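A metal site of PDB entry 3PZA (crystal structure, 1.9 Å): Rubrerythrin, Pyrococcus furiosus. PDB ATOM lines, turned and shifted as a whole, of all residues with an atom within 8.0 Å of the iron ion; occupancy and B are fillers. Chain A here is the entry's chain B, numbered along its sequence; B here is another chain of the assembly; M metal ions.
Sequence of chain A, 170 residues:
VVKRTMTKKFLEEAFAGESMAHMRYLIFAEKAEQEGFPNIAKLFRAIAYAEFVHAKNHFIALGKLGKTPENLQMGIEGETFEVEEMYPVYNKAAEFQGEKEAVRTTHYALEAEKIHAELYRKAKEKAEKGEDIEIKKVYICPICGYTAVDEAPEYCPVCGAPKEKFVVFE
The side-chain sulfur of Cys 159 sits close to the backbone NH of Ala 161. N of Tyr 146 lies close to SG of Cys 144. The side-chain sulfur (SG) of Cys 141 lies close to the backbone NH (N) of Ile 143, at 3.5 Å. The backbone NH (N) of Cys 156 sits at hydrogen-bond distance from the backbone carbonyl oxygen (O) of Ala 161, at 2.6 Å. N of Cys 141 is in hydrogen-bond range of O of Tyr 146, 2.8 Å away. The side-chain sulfur (SG) of Cys 156 sits close to the backbone NH (N) of Val 158 (3.5 Å).
Four residues have an atom within 4 Å of the iron ion: Cys 141, Cys 144, Cys 156 and Cys 159. Along chain A the residues within 4 Å of the iron ion span positions 141 to 159.
The iron ion is bound by SG of Cys 159 (2.3 Å). SG of Cys 141 binds the iron ion (2.3 Å). The iron ion is bound by SG of Cys 156, 2.3 Å away. The iron ion is bound by SG of Cys 144, at 2.3 Å. The iron ion has four donor atoms within binding distance.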
ATOM      1  N   TYR A 108      14.367  -4.691  -4.840  1.00  0.00           N
ATOM      2  CA  TYR A 108      13.589  -4.413  -6.015  1.00  0.00           C
ATOM      3  C   TYR A 108      12.469  -3.377  -5.778  1.00  0.00           C
ATOM      4  O   TYR A 108      12.198  -2.460  -6.586  1.00  0.00           O
ATOM      5  CB  TYR A 108      12.945  -5.736  -6.446  1.00  0.00           C
ATOM      6  CG  TYR A 108      13.768  -6.785  -7.128  1.00  0.00           C
ATOM      7  CD1 TYR A 108      15.071  -6.506  -7.567  1.00  0.00           C
ATOM      8  CD2 TYR A 108      13.169  -8.025  -7.459  1.00  0.00           C
ATOM      9  CE1 TYR A 108      15.814  -7.453  -8.267  1.00  0.00           C
ATOM     10  CE2 TYR A 108      13.874  -8.996  -8.098  1.00  0.00           C
ATOM     11  CZ  TYR A 108      15.203  -8.683  -8.587  1.00  0.00           C
ATOM     12  OH  TYR A 108      15.958  -9.649  -9.278  1.00  0.00           O
ATOM     13  N   ILE A 140       6.764  -1.314 -17.571  1.00  0.00           N
ATOM     14  CA  ILE A 140       7.017  -1.845 -16.249  1.00  0.00           C
ATOM     15  C   ILE A 140       7.773  -3.148 -16.342  1.00  0.00           C
ATOM     16  O   ILE A 140       7.383  -4.032 -17.093  1.00  0.00           O
ATOM     17  CB  ILE A 140       5.614  -2.178 -15.459  1.00  0.00           C
ATOM     18  CG1 ILE A 140       4.706  -0.969 -15.374  1.00  0.00           C
ATOM     19  CG2 ILE A 140       5.949  -2.713 -14.008  1.00  0.00           C
ATOM     20  CD1 ILE A 140       5.340   0.299 -14.604  1.00  0.00           C
ATOM     21  N   CYS A 141       8.922  -3.287 -15.642  1.00  0.00           N
ATOM     22  CA  CYS A 141       9.599  -4.579 -15.593  1.00  0.00           C
ATOM     23  C   CYS A 141       8.768  -5.640 -14.799  1.00  0.00           C
ATOM     24  O   CYS A 141       8.401  -5.395 -13.650  1.00  0.00           O
ATOM     25  CB  CYS A 141      10.929  -4.398 -14.893  1.00  0.00           C
ATOM     26  SG  CYS A 141      11.867  -5.906 -14.851  1.00  0.00           S
ATOM     27  N   PRO A 142       8.488  -6.806 -15.414  1.00  0.00           N
ATOM     28  CA  PRO A 142       7.623  -7.840 -14.748  1.00  0.00           C
ATOM     29  C   PRO A 142       8.428  -8.637 -13.748  1.00  0.00           C
ATOM     30  O   PRO A 142       7.870  -9.410 -13.015  1.00  0.00           O
ATOM     31  CB  PRO A 142       7.156  -8.717 -15.918  1.00  0.00           C
ATOM     32  CG  PRO A 142       8.411  -8.657 -16.938  1.00  0.00           C
ATOM     33  CD  PRO A 142       8.808  -7.123 -16.842  1.00  0.00           C
ATOM     34  N   ILE A 143       9.752  -8.390 -13.657  1.00  0.00           N
ATOM     35  CA  ILE A 143      10.615  -9.061 -12.657  1.00  0.00           C
ATOM     36  C   ILE A 143      10.723  -8.291 -11.332  1.00  0.00           C
ATOM     37  O   ILE A 143      10.562  -8.849 -10.223  1.00  0.00           O
ATOM     38  CB  ILE A 143      12.060  -9.230 -13.191  1.00  0.00           C
ATOM     39  CG1 ILE A 143      12.065  -9.929 -14.568  1.00  0.00           C
ATOM     40  CG2 ILE A 143      12.914 -10.002 -12.142  1.00  0.00           C
ATOM     41  CD1 ILE A 143      11.524 -11.326 -14.680  1.00  0.00           C
ATOM     42  N   CYS A 144      10.939  -6.993 -11.404  1.00  0.00           N
ATOM     43  CA  CYS A 144      11.212  -6.185 -10.212  1.00  0.00           C
ATOM     44  C   CYS A 144      10.293  -4.958 -10.097  1.00  0.00           C
ATOM     45  O   CYS A 144      10.318  -4.222  -9.081  1.00  0.00           O
ATOM     46  CB  CYS A 144      12.697  -5.743 -10.182  1.00  0.00           C
ATOM     47  SG  CYS A 144      13.046  -4.441 -11.437  1.00  0.00           S
ATOM     48  N   GLY A 145       9.491  -4.623 -11.131  1.00  0.00           N
ATOM     49  CA  GLY A 145       8.591  -3.475 -10.917  1.00  0.00           C
ATOM     50  C   GLY A 145       9.202  -2.157 -11.336  1.00  0.00           C
ATOM     51  O   GLY A 145       8.603  -1.130 -11.238  1.00  0.00           O
ATOM     52  N   TYR A 146      10.453  -2.184 -11.807  1.00  0.00           N
ATOM     53  CA  TYR A 146      11.061  -0.946 -12.266  1.00  0.00           C
ATOM     54  C   TYR A 146      10.145  -0.259 -13.306  1.00  0.00           C
ATOM     55  O   TYR A 146       9.633  -0.932 -14.203  1.00  0.00           O
ATOM     56  CB  TYR A 146      12.430  -1.291 -12.932  1.00  0.00           C
ATOM     57  CG  TYR A 146      13.065  -0.029 -13.462  1.00  0.00           C
ATOM     58  CD1 TYR A 146      13.711   0.817 -12.535  1.00  0.00           C
ATOM     59  CD2 TYR A 146      13.117   0.260 -14.800  1.00  0.00           C
ATOM     60  CE1 TYR A 146      14.319   1.964 -12.925  1.00  0.00           C
ATOM     61  CE2 TYR A 146      13.767   1.482 -15.231  1.00  0.00           C
ATOM     62  CZ  TYR A 146      14.338   2.280 -14.273  1.00  0.00           C
ATOM     63  OH  TYR A 146      14.967   3.438 -14.574  1.00  0.00           O
ATOM     64  N   THR A 147      10.000   1.062 -13.223  1.00  0.00           N
ATOM     65  CA  THR A 147       8.964   1.804 -13.930  1.00  0.00           C
ATOM     66  C   THR A 147       9.671   2.884 -14.772  1.00  0.00           C
ATOM     67  O   THR A 147      10.523   3.623 -14.240  1.00  0.00           O
ATOM     68  CB  THR A 147       8.080   2.493 -12.900  1.00  0.00           C
ATOM     69  OG1 THR A 147       7.439   1.440 -12.138  1.00  0.00           O
ATOM     70  CG2 THR A 147       7.029   3.394 -13.565  1.00  0.00           C
ATOM     71  N   TYR A 155      18.152  -2.213 -20.883  1.00  0.00           N
ATOM     72  CA  TYR A 155      17.953  -3.346 -19.950  1.00  0.00           C
ATOM     73  C   TYR A 155      17.504  -2.739 -18.637  1.00  0.00           C
ATOM     74  O   TYR A 155      17.756  -1.552 -18.371  1.00  0.00           O
ATOM     75  CB  TYR A 155      19.257  -4.128 -19.757  1.00  0.00           C
ATOM     76  CG  TYR A 155      20.437  -3.338 -19.140  1.00  0.00           C
ATOM     77  CD1 TYR A 155      20.582  -3.268 -17.761  1.00  0.00           C
ATOM     78  CD2 TYR A 155      21.448  -2.701 -19.951  1.00  0.00           C
ATOM     79  CE1 TYR A 155      21.687  -2.535 -17.133  1.00  0.00           C
ATOM     80  CE2 TYR A 155      22.564  -1.968 -19.313  1.00  0.00           C
ATOM     81  CZ  TYR A 155      22.651  -1.923 -17.924  1.00  0.00           C
ATOM     82  OH  TYR A 155      23.694  -1.258 -17.185  1.00  0.00           O
ATOM     83  N   CYS A 156      16.819  -3.536 -17.812  1.00  0.00           N
ATOM     84  CA  CYS A 156      16.369  -3.029 -16.501  1.00  0.00           C
ATOM     85  C   CYS A 156      17.571  -2.733 -15.577  1.00  0.00           C
ATOM     86  O   CYS A 156      18.371  -3.603 -15.318  1.00  0.00           O
ATOM     87  CB  CYS A 156      15.427  -4.100 -15.824  1.00  0.00           C
ATOM     88  SG  CYS A 156      14.907  -3.443 -14.210  1.00  0.00           S
ATOM     89  N   PRO A 157      17.751  -1.504 -15.120  1.00  0.00           N
ATOM     90  CA  PRO A 157      18.969  -1.276 -14.248  1.00  0.00           C
ATOM     91  C   PRO A 157      18.963  -1.943 -12.883  1.00  0.00           C
ATOM     92  O   PRO A 157      20.030  -2.059 -12.191  1.00  0.00           O
ATOM     93  CB  PRO A 157      19.034   0.266 -14.116  1.00  0.00           C
ATOM     94  CG  PRO A 157      17.541   0.636 -14.219  1.00  0.00           C
ATOM     95  CD  PRO A 157      17.015  -0.246 -15.348  1.00  0.00           C
ATOM     96  N   VAL A 158      17.764  -2.353 -12.437  1.00  0.00           N
ATOM     97  CA  VAL A 158      17.693  -2.986 -11.151  1.00  0.00           C
ATOM     98  C   VAL A 158      17.905  -4.472 -11.207  1.00  0.00           C
ATOM     99  O   VAL A 158      18.575  -5.039 -10.342  1.00  0.00           O
ATOM    100  CB  VAL A 158      16.307  -2.682 -10.526  1.00  0.00           C
ATOM    101  CG1 VAL A 158      16.058  -3.432  -9.198  1.00  0.00           C
ATOM    102  CG2 VAL A 158      16.209  -1.105 -10.401  1.00  0.00           C
ATOM    103  N   CYS A 159      17.323  -5.161 -12.163  1.00  0.00           N
ATOM    104  CA  CYS A 159      17.463  -6.625 -12.127  1.00  0.00           C
ATOM    105  C   CYS A 159      18.191  -7.186 -13.364  1.00  0.00           C
ATOM    106  O   CYS A 159      18.405  -8.380 -13.437  1.00  0.00           O
ATOM    107  CB  CYS A 159      16.101  -7.297 -12.121  1.00  0.00           C
ATOM    108  SG  CYS A 159      14.994  -7.198 -13.572  1.00  0.00           S
ATOM    109  N   GLY A 160      18.366  -6.336 -14.350  1.00  0.00           N
ATOM    110  CA  GLY A 160      19.106  -6.705 -15.585  1.00  0.00           C
ATOM    111  C   GLY A 160      18.236  -7.259 -16.746  1.00  0.00           C
ATOM    112  O   GLY A 160      18.752  -7.580 -17.857  1.00  0.00           O
ATOM    113  N   ALA A 161      16.906  -7.297 -16.575  1.00  0.00           N
ATOM    114  CA  ALA A 161      16.035  -7.812 -17.635  1.00  0.00           C
ATOM    115  C   ALA A 161      16.119  -7.007 -18.940  1.00  0.00           C
ATOM    116  O   ALA A 161      16.127  -5.731 -18.949  1.00  0.00           O
ATOM    117  CB  ALA A 161      14.544  -7.779 -17.080  1.00  0.00           C
ATOM    118  N   PRO A 162      16.017  -7.709 -20.104  1.00  0.00           N
ATOM    119  CA  PRO A 162      16.020  -7.003 -21.399  1.00  0.00           C
ATOM    120  C   PRO A 162      14.802  -6.182 -21.662  1.00  0.00           C
ATOM    121  O   PRO A 162      13.706  -6.503 -21.147  1.00  0.00           O
ATOM    122  CB  PRO A 162      16.115  -8.159 -22.440  1.00  0.00           C
ATOM    123  CG  PRO A 162      15.561  -9.303 -21.760  1.00  0.00           C
ATOM    124  CD  PRO A 162      15.963  -9.159 -20.255  1.00  0.00           C
ATOM    125  N   LYS A 165      11.319  -7.583 -22.367  1.00  0.00           N
ATOM    126  CA  LYS A 165      10.475  -8.146 -21.268  1.00  0.00           C
ATOM    127  C   LYS A 165       9.546  -7.156 -20.645  1.00  0.00           C
ATOM    128  O   LYS A 165       8.583  -7.586 -19.952  1.00  0.00           O
ATOM    129  CB  LYS A 165      11.362  -8.726 -20.117  1.00  0.00           C
ATOM    130  CG  LYS A 165      12.175  -9.931 -20.460  1.00  0.00           C
ATOM    131  CD  LYS A 165      11.347 -11.120 -20.977  1.00  0.00           C
ATOM    132  CE  LYS A 165      12.230 -12.391 -21.062  1.00  0.00           C
ATOM    133  NZ  LYS A 165      12.020 -13.131 -22.355  1.00  0.00           N
ATOM    134  N   PHE A 166       9.790  -5.855 -20.848  1.00  0.00           N
ATOM    135  CA  PHE A 166       8.930  -4.848 -20.225  1.00  0.00           C
ATOM    136  C   PHE A 166       7.483  -4.921 -20.693  1.00  0.00           C
ATOM    137  O   PHE A 166       7.200  -5.198 -21.871  1.00  0.00           O
ATOM    138  CB  PHE A 166       9.453  -3.420 -20.432  1.00  0.00           C
ATOM    139  CG  PHE A 166      10.617  -3.046 -19.518  1.00  0.00           C
ATOM    140  CD1 PHE A 166      10.390  -2.175 -18.407  1.00  0.00           C
ATOM    141  CD2 PHE A 166      11.911  -3.483 -19.762  1.00  0.00           C
ATOM    142  CE1 PHE A 166      11.475  -1.819 -17.531  1.00  0.00           C
ATOM    143  CE2 PHE A 166      13.027  -3.134 -18.878  1.00  0.00           C
ATOM    144  CZ  PHE A 166      12.810  -2.271 -17.827  1.00  0.00           C
ATOM    145  N   VAL B  53       3.855  -6.708  -9.067  1.00  0.00           N
ATOM    146  CA  VAL B  53       5.102  -7.362  -9.142  1.00  0.00           C
ATOM    147  C   VAL B  53       5.793  -7.430  -7.764  1.00  0.00           C
ATOM    148  O   VAL B  53       6.344  -8.506  -7.382  1.00  0.00           O
ATOM    149  CB  VAL B  53       6.005  -6.682 -10.222  1.00  0.00           C
ATOM    150  CG1 VAL B  53       7.359  -7.397 -10.259  1.00  0.00           C
ATOM    151  CG2 VAL B  53       5.333  -6.823 -11.652  1.00  0.00           C
HETATM  152 FE    FE M   1      13.679  -5.305 -13.515  1.00  0.00          FE
